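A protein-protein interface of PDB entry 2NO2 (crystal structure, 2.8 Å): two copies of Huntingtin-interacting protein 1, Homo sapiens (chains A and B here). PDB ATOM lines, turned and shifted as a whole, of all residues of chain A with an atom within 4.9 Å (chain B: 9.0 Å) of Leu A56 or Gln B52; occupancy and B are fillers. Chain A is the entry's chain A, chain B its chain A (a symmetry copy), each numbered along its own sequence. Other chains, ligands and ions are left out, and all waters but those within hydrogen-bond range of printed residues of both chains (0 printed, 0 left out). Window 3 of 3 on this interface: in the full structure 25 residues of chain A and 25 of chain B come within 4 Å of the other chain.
CD1 of Leu B56 touches NE2 of Gln A52 (3.2 Å).
Gln B52 touches Leu A56.
CD2 of Leu A59 touches CG of Lys B60, at 3.9 Å.
Leu A59 touches Leu B63.
Lys A60 touches Leu B59.
Gln A52 touches Leu B56, and with the chains exchanged Leu A56 touches Gln B52.
Leu A59 touches Lys B60, and with the chains exchanged Lys A60 touches Leu B59.
Of the 5 pairs that touch across the chains among the printed residues, 4 have their exchanged pair printed and touching as well.
Of the 17 printed residues of chain B, 5 touch a printed residue of chain A.
Hydrophobic or aromatic side chains of chain B within 4 Å of the printed part of chain A: Leu B56, Leu B59 and Leu B63.
Printed residues of chain A that touch a printed residue of chain B: Gln A52, Leu A56, Leu A59 and Lys A60.
Hydrophobic or aromatic side chains of chain A within 4 Å of the printed part of chain B: Leu A56 and Leu A59.
Leu A56 touches just one residue of chain B: Gln B52 (3.2 Å).
Of the printed residues of chain A, Gln B52 touches Leu A56.
No residue of chain B comes within 4 Å of Val A55.
Of the printed residues of chain A, Leu B59 touches Lys A60.
Of the printed residues of chain A, Lys B60 touches Leu A59 (3.9 Å).
Lys B48 touches none of the printed residues of chain A.
The nearest residue of chain B that does not touch Leu A56 is Leu B59 (4.6 Å).
The nearest printed residue of chain A that does not touch Gln B52 is Gln A52 (6.4 Å).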
ATOM      1  N   GLN A  52      28.098  -5.996 -21.886  1.00  0.00           N
ATOM      2  CA  GLN A  52      28.264  -5.107 -20.746  1.00  0.00           C
ATOM      3  C   GLN A  52      27.147  -4.053 -20.704  1.00  0.00           C
ATOM      4  O   GLN A  52      26.446  -3.909 -19.687  1.00  0.00           O
ATOM      5  CB  GLN A  52      29.636  -4.438 -20.822  1.00  0.00           C
ATOM      6  CG  GLN A  52      30.027  -3.650 -19.596  1.00  0.00           C
ATOM      7  CD  GLN A  52      29.770  -4.419 -18.326  1.00  0.00           C
ATOM      8  OE1 GLN A  52      29.961  -5.632 -18.278  1.00  0.00           O
ATOM      9  NE2 GLN A  52      29.344  -3.717 -17.283  1.00  0.00           N
ATOM     10  N   LEU A  53      26.968  -3.323 -21.803  1.00  0.00           N
ATOM     11  CA  LEU A  53      25.914  -2.313 -21.860  1.00  0.00           C
ATOM     12  C   LEU A  53      24.553  -2.930 -21.511  1.00  0.00           C
ATOM     13  O   LEU A  53      23.724  -2.280 -20.883  1.00  0.00           O
ATOM     14  CB  LEU A  53      25.858  -1.678 -23.251  1.00  0.00           C
ATOM     15  CG  LEU A  53      27.127  -0.939 -23.688  1.00  0.00           C
ATOM     16  CD1 LEU A  53      27.075  -0.662 -25.186  1.00  0.00           C
ATOM     17  CD2 LEU A  53      27.275   0.354 -22.915  1.00  0.00           C
ATOM     18  N   GLU A  54      24.338  -4.183 -21.911  1.00  0.00           N
ATOM     19  CA  GLU A  54      23.091  -4.885 -21.635  1.00  0.00           C
ATOM     20  C   GLU A  54      23.041  -5.348 -20.179  1.00  0.00           C
ATOM     21  O   GLU A  54      21.951  -5.509 -19.596  1.00  0.00           O
ATOM     22  CB  GLU A  54      22.932  -6.082 -22.573  1.00  0.00           C
ATOM     23  CG  GLU A  54      22.832  -5.682 -24.032  1.00  0.00           C
ATOM     24  CD  GLU A  54      22.665  -6.864 -24.958  1.00  0.00           C
ATOM     25  OE1 GLU A  54      23.539  -7.760 -24.956  1.00  0.00           O
ATOM     26  OE2 GLU A  54      21.658  -6.890 -25.695  1.00  0.00           O
ATOM     27  N   VAL A  55      24.210  -5.561 -19.574  1.00  0.00           N
ATOM     28  CA  VAL A  55      24.253  -5.984 -18.174  1.00  0.00           C
ATOM     29  C   VAL A  55      23.939  -4.779 -17.304  1.00  0.00           C
ATOM     30  O   VAL A  55      23.172  -4.862 -16.354  1.00  0.00           O
ATOM     31  CB  VAL A  55      25.638  -6.529 -17.792  1.00  0.00           C
ATOM     32  CG1 VAL A  55      25.682  -6.852 -16.316  1.00  0.00           C
ATOM     33  CG2 VAL A  55      25.923  -7.767 -18.589  1.00  0.00           C
ATOM     34  N   LEU A  56      24.536  -3.650 -17.663  1.00  0.00           N
ATOM     35  CA  LEU A  56      24.332  -2.413 -16.934  1.00  0.00           C
ATOM     36  C   LEU A  56      22.883  -1.942 -17.023  1.00  0.00           C
ATOM     37  O   LEU A  56      22.314  -1.469 -16.038  1.00  0.00           O
ATOM     38  CB  LEU A  56      25.278  -1.345 -17.475  1.00  0.00           C
ATOM     39  CG  LEU A  56      25.092   0.058 -16.913  1.00  0.00           C
ATOM     40  CD1 LEU A  56      26.442   0.719 -16.802  1.00  0.00           C
ATOM     41  CD2 LEU A  56      24.159   0.865 -17.810  1.00  0.00           C
ATOM     42  N   GLU A  57      22.292  -2.072 -18.206  1.00  0.00           N
ATOM     43  CA  GLU A  57      20.914  -1.661 -18.407  1.00  0.00           C
ATOM     44  C   GLU A  57      20.003  -2.543 -17.581  1.00  0.00           C
ATOM     45  O   GLU A  57      19.156  -2.058 -16.836  1.00  0.00           O
ATOM     46  CB  GLU A  57      20.523  -1.782 -19.870  1.00  0.00           C
ATOM     47  CG  GLU A  57      19.110  -1.318 -20.140  1.00  0.00           C
ATOM     48  CD  GLU A  57      18.821   0.022 -19.488  1.00  0.00           C
ATOM     49  OE1 GLU A  57      19.790   0.776 -19.222  1.00  0.00           O
ATOM     50  OE2 GLU A  57      17.629   0.321 -19.251  1.00  0.00           O
ATOM     51  N   SER A  58      20.180  -3.849 -17.720  1.00  0.00           N
ATOM     52  CA  SER A  58      19.383  -4.809 -16.977  1.00  0.00           C
ATOM     53  C   SER A  58      19.506  -4.577 -15.467  1.00  0.00           C
ATOM     54  O   SER A  58      18.508  -4.588 -14.734  1.00  0.00           O
ATOM     55  CB  SER A  58      19.838  -6.220 -17.323  1.00  0.00           C
ATOM     56  OG  SER A  58      19.207  -7.155 -16.470  1.00  0.00           O
ATOM     57  N   LEU A  59      20.738  -4.372 -15.009  1.00  0.00           N
ATOM     58  CA  LEU A  59      21.026  -4.133 -13.597  1.00  0.00           C
ATOM     59  C   LEU A  59      20.157  -2.995 -13.061  1.00  0.00           C
ATOM     60  O   LEU A  59      19.525  -3.141 -12.021  1.00  0.00           O
ATOM     61  CB  LEU A  59      22.511  -3.808 -13.433  1.00  0.00           C
ATOM     62  CG  LEU A  59      23.148  -4.134 -12.090  1.00  0.00           C
ATOM     63  CD1 LEU A  59      22.669  -5.471 -11.593  1.00  0.00           C
ATOM     64  CD2 LEU A  59      24.649  -4.151 -12.253  1.00  0.00           C
ATOM     65  N   LYS A  60      20.112  -1.875 -13.779  1.00  0.00           N
ATOM     66  CA  LYS A  60      19.286  -0.749 -13.361  1.00  0.00           C
ATOM     67  C   LYS A  60      17.832  -1.202 -13.306  1.00  0.00           C
ATOM     68  O   LYS A  60      17.128  -0.951 -12.322  1.00  0.00           O
ATOM     69  CB  LYS A  60      19.417   0.405 -14.346  1.00  0.00           C
ATOM     70  CG  LYS A  60      20.823   0.935 -14.469  1.00  0.00           C
ATOM     71  CD  LYS A  60      20.915   1.940 -15.591  1.00  0.00           C
ATOM     72  CE  LYS A  60      22.306   2.529 -15.695  1.00  0.00           C
ATOM     73  NZ  LYS A  60      22.438   3.470 -16.856  1.00  0.00           N
ATOM     74  N   GLY B  45      39.401  11.588 -19.012  1.00  0.00           N
ATOM     75  CA  GLY B  45      38.967  10.281 -19.472  1.00  0.00           C
ATOM     76  C   GLY B  45      39.282   9.126 -18.538  1.00  0.00           C
ATOM     77  O   GLY B  45      38.563   8.129 -18.505  1.00  0.00           O
ATOM     78  N   GLN B  46      40.359   9.247 -17.776  1.00  0.00           N
ATOM     79  CA  GLN B  46      40.728   8.183 -16.867  1.00  0.00           C
ATOM     80  C   GLN B  46      39.916   8.243 -15.579  1.00  0.00           C
ATOM     81  O   GLN B  46      39.776   7.237 -14.880  1.00  0.00           O
ATOM     82  CB  GLN B  46      42.217   8.256 -16.560  1.00  0.00           C
ATOM     83  CG  GLN B  46      42.710   7.111 -15.714  1.00  0.00           C
ATOM     84  CD  GLN B  46      43.973   6.495 -16.266  1.00  0.00           C
ATOM     85  OE1 GLN B  46      43.962   5.872 -17.331  1.00  0.00           O
ATOM     86  NE2 GLN B  46      45.078   6.671 -15.549  1.00  0.00           N
ATOM     87  N   ARG B  47      39.377   9.417 -15.259  1.00  0.00           N
ATOM     88  CA  ARG B  47      38.578   9.549 -14.049  1.00  0.00           C
ATOM     89  C   ARG B  47      37.141   9.149 -14.353  1.00  0.00           C
ATOM     90  O   ARG B  47      36.430   8.679 -13.472  1.00  0.00           O
ATOM     91  CB  ARG B  47      38.618  10.979 -13.506  1.00  0.00           C
ATOM     92  CG  ARG B  47      37.608  11.917 -14.136  1.00  0.00           C
ATOM     93  CD  ARG B  47      37.762  13.320 -13.594  1.00  0.00           C
ATOM     94  NE  ARG B  47      39.145  13.777 -13.711  1.00  0.00           N
ATOM     95  CZ  ARG B  47      39.536  15.037 -13.552  1.00  0.00           C
ATOM     96  NH1 ARG B  47      38.645  15.978 -13.270  1.00  0.00           N
ATOM     97  NH2 ARG B  47      40.817  15.358 -13.680  1.00  0.00           N
ATOM     98  N   LYS B  48      36.706   9.339 -15.596  1.00  0.00           N
ATOM     99  CA  LYS B  48      35.349   8.956 -15.963  1.00  0.00           C
ATOM    100  C   LYS B  48      35.252   7.440 -15.936  1.00  0.00           C
ATOM    101  O   LYS B  48      34.227   6.876 -15.554  1.00  0.00           O
ATOM    102  CB  LYS B  48      34.987   9.484 -17.348  1.00  0.00           C
ATOM    103  CG  LYS B  48      34.596  10.941 -17.338  1.00  0.00           C
ATOM    104  CD  LYS B  48      33.762  11.276 -18.549  1.00  0.00           C
ATOM    105  CE  LYS B  48      33.054  12.598 -18.362  1.00  0.00           C
ATOM    106  NZ  LYS B  48      32.016  12.811 -19.407  1.00  0.00           N
ATOM    107  N   THR B  49      36.335   6.788 -16.341  1.00  0.00           N
ATOM    108  CA  THR B  49      36.413   5.336 -16.334  1.00  0.00           C
ATOM    109  C   THR B  49      36.264   4.846 -14.893  1.00  0.00           C
ATOM    110  O   THR B  49      35.694   3.791 -14.642  1.00  0.00           O
ATOM    111  CB  THR B  49      37.762   4.870 -16.909  1.00  0.00           C
ATOM    112  OG1 THR B  49      37.770   5.105 -18.319  1.00  0.00           O
ATOM    113  CG2 THR B  49      37.994   3.396 -16.652  1.00  0.00           C
ATOM    114  N   GLN B  50      36.780   5.620 -13.947  1.00  0.00           N
ATOM    115  CA  GLN B  50      36.683   5.259 -12.543  1.00  0.00           C
ATOM    116  C   GLN B  50      35.262   5.401 -12.023  1.00  0.00           C
ATOM    117  O   GLN B  50      34.658   4.428 -11.590  1.00  0.00           O
ATOM    118  CB  GLN B  50      37.618   6.123 -11.709  1.00  0.00           C
ATOM    119  CG  GLN B  50      38.923   5.454 -11.457  1.00  0.00           C
ATOM    120  CD  GLN B  50      38.712   4.062 -10.927  1.00  0.00           C
ATOM    121  OE1 GLN B  50      37.945   3.858  -9.982  1.00  0.00           O
ATOM    122  NE2 GLN B  50      39.385   3.090 -11.531  1.00  0.00           N
ATOM    123  N   GLU B  51      34.731   6.618 -12.064  1.00  0.00           N
ATOM    124  CA  GLU B  51      33.378   6.866 -11.598  1.00  0.00           C
ATOM    125  C   GLU B  51      32.476   5.738 -12.060  1.00  0.00           C
ATOM    126  O   GLU B  51      31.705   5.191 -11.275  1.00  0.00           O
ATOM    127  CB  GLU B  51      32.863   8.182 -12.158  1.00  0.00           C
ATOM    128  CG  GLU B  51      33.822   9.327 -11.974  1.00  0.00           C
ATOM    129  CD  GLU B  51      33.304  10.597 -12.597  1.00  0.00           C
ATOM    130  OE1 GLU B  51      34.100  11.550 -12.757  1.00  0.00           O
ATOM    131  OE2 GLU B  51      32.095  10.636 -12.920  1.00  0.00           O
ATOM    132  N   GLN B  52      32.579   5.387 -13.335  1.00  0.00           N
ATOM    133  CA  GLN B  52      31.766   4.319 -13.899  1.00  0.00           C
ATOM    134  C   GLN B  52      31.961   3.011 -13.118  1.00  0.00           C
ATOM    135  O   GLN B  52      30.987   2.404 -12.641  1.00  0.00           O
ATOM    136  CB  GLN B  52      32.130   4.131 -15.370  1.00  0.00           C
ATOM    137  CG  GLN B  52      31.221   3.199 -16.135  1.00  0.00           C
ATOM    138  CD  GLN B  52      29.766   3.496 -15.878  1.00  0.00           C
ATOM    139  OE1 GLN B  52      29.375   4.653 -15.747  1.00  0.00           O
ATOM    140  NE2 GLN B  52      28.950   2.450 -15.813  1.00  0.00           N
ATOM    141  N   LEU B  53      33.212   2.577 -12.975  1.00  0.00           N
ATOM    142  CA  LEU B  53      33.493   1.353 -12.228  1.00  0.00           C
ATOM    143  C   LEU B  53      32.885   1.426 -10.821  1.00  0.00           C
ATOM    144  O   LEU B  53      32.422   0.419 -10.296  1.00  0.00           O
ATOM    145  CB  LEU B  53      35.001   1.120 -12.133  1.00  0.00           C
ATOM    146  CG  LEU B  53      35.723   0.931 -13.472  1.00  0.00           C
ATOM    147  CD1 LEU B  53      37.228   1.056 -13.270  1.00  0.00           C
ATOM    148  CD2 LEU B  53      35.378  -0.416 -14.069  1.00  0.00           C
ATOM    149  N   GLU B  54      32.881   2.619 -10.226  1.00  0.00           N
ATOM    150  CA  GLU B  54      32.326   2.823  -8.894  1.00  0.00           C
ATOM    151  C   GLU B  54      30.798   2.849  -8.942  1.00  0.00           C
ATOM    152  O   GLU B  54      30.120   2.522  -7.949  1.00  0.00           O
ATOM    153  CB  GLU B  54      32.855   4.121  -8.287  1.00  0.00           C
ATOM    154  CG  GLU B  54      34.357   4.109  -8.078  1.00  0.00           C
ATOM    155  CD  GLU B  54      34.879   5.389  -7.469  1.00  0.00           C
ATOM    156  OE1 GLU B  54      34.672   6.469  -8.066  1.00  0.00           O
ATOM    157  OE2 GLU B  54      35.504   5.310  -6.392  1.00  0.00           O
ATOM    158  N   VAL B  55      30.239   3.230 -10.091  1.00  0.00           N
ATOM    159  CA  VAL B  55      28.782   3.263 -10.231  1.00  0.00           C
ATOM    160  C   VAL B  55      28.288   1.834 -10.379  1.00  0.00           C
ATOM    161  O   VAL B  55      27.305   1.434  -9.769  1.00  0.00           O
ATOM    162  CB  VAL B  55      28.351   4.071 -11.464  1.00  0.00           C
ATOM    163  CG1 VAL B  55      26.853   3.992 -11.643  1.00  0.00           C
ATOM    164  CG2 VAL B  55      28.765   5.503 -11.290  1.00  0.00           C
ATOM    165  N   LEU B  56      29.003   1.069 -11.192  1.00  0.00           N
ATOM    166  CA  LEU B  56      28.660  -0.320 -11.433  1.00  0.00           C
ATOM    167  C   LEU B  56      28.785  -1.157 -10.163  1.00  0.00           C
ATOM    168  O   LEU B  56      27.948  -2.019  -9.893  1.00  0.00           O
ATOM    169  CB  LEU B  56      29.556  -0.879 -12.535  1.00  0.00           C
ATOM    170  CG  LEU B  56      29.422  -2.371 -12.811  1.00  0.00           C
ATOM    171  CD1 LEU B  56      29.604  -2.608 -14.288  1.00  0.00           C
ATOM    172  CD2 LEU B  56      30.452  -3.151 -12.000  1.00  0.00           C
ATOM    173  N   GLU B  57      29.834  -0.900  -9.388  1.00  0.00           N
ATOM    174  CA  GLU B  57      30.052  -1.632  -8.153  1.00  0.00           C
ATOM    175  C   GLU B  57      28.943  -1.309  -7.176  1.00  0.00           C
ATOM    176  O   GLU B  57      28.318  -2.200  -6.609  1.00  0.00           O
ATOM    177  CB  GLU B  57      31.385  -1.251  -7.529  1.00  0.00           C
ATOM    178  CG  GLU B  57      31.683  -2.023  -6.264  1.00  0.00           C
ATOM    179  CD  GLU B  57      31.437  -3.510  -6.440  1.00  0.00           C
ATOM    180  OE1 GLU B  57      31.473  -3.987  -7.602  1.00  0.00           O
ATOM    181  OE2 GLU B  57      31.218  -4.200  -5.418  1.00  0.00           O
ATOM    182  N   SER B  58      28.702  -0.020  -6.980  1.00  0.00           N
ATOM    183  CA  SER B  58      27.656   0.430  -6.079  1.00  0.00           C
ATOM    184  C   SER B  58      26.294  -0.144  -6.483  1.00  0.00           C
ATOM    185  O   SER B  58      25.524  -0.622  -5.640  1.00  0.00           O
ATOM    186  CB  SER B  58      27.600   1.952  -6.089  1.00  0.00           C
ATOM    187  OG  SER B  58      26.468   2.399  -5.370  1.00  0.00           O
ATOM    188  N   LEU B  59      26.002  -0.089  -7.781  1.00  0.00           N
ATOM    189  CA  LEU B  59      24.747  -0.596  -8.330  1.00  0.00           C
ATOM    190  C   LEU B  59      24.512  -2.038  -7.882  1.00  0.00           C
ATOM    191  O   LEU B  59      23.435  -2.365  -7.397  1.00  0.00           O
ATOM    192  CB  LEU B  59      24.788  -0.498  -9.855  1.00  0.00           C
ATOM    193  CG  LEU B  59      23.455  -0.366 -10.578  1.00  0.00           C
ATOM    194  CD1 LEU B  59      22.555   0.590  -9.843  1.00  0.00           C
ATOM    195  CD2 LEU B  59      23.708   0.137 -11.979  1.00  0.00           C
ATOM    196  N   LYS B  60      25.525  -2.891  -8.026  1.00  0.00           N
ATOM    197  CA  LYS B  60      25.402  -4.280  -7.598  1.00  0.00           C
ATOM    198  C   LYS B  60      25.117  -4.307  -6.102  1.00  0.00           C
ATOM    199  O   LYS B  60      24.206  -5.005  -5.645  1.00  0.00           O
ATOM    200  CB  LYS B  60      26.690  -5.041  -7.880  1.00  0.00           C
ATOM    201  CG  LYS B  60      27.061  -5.080  -9.340  1.00  0.00           C
ATOM    202  CD  LYS B  60      28.433  -5.680  -9.525  1.00  0.00           C
ATOM    203  CE  LYS B  60      28.801  -5.783 -10.990  1.00  0.00           C
ATOM    204  NZ  LYS B  60      30.194  -6.302 -11.190  1.00  0.00           N
ATOM    205  N   LEU B  63      21.470  -3.307  -5.371  1.00  0.00           N
ATOM    206  CA  LEU B  63      20.538  -4.373  -5.723  1.00  0.00           C
ATOM    207  C   LEU B  63      20.588  -5.503  -4.714  1.00  0.00           C
ATOM    208  O   LEU B  63      19.548  -5.989  -4.284  1.00  0.00           O
ATOM    209  CB  LEU B  63      20.848  -4.929  -7.114  1.00  0.00           C
ATOM    210  CG  LEU B  63      19.978  -6.092  -7.588  1.00  0.00           C
ATOM    211  CD1 LEU B  63      18.528  -5.796  -7.301  1.00  0.00           C
ATOM    212  CD2 LEU B  63      20.183  -6.315  -9.072  1.00  0.00           C
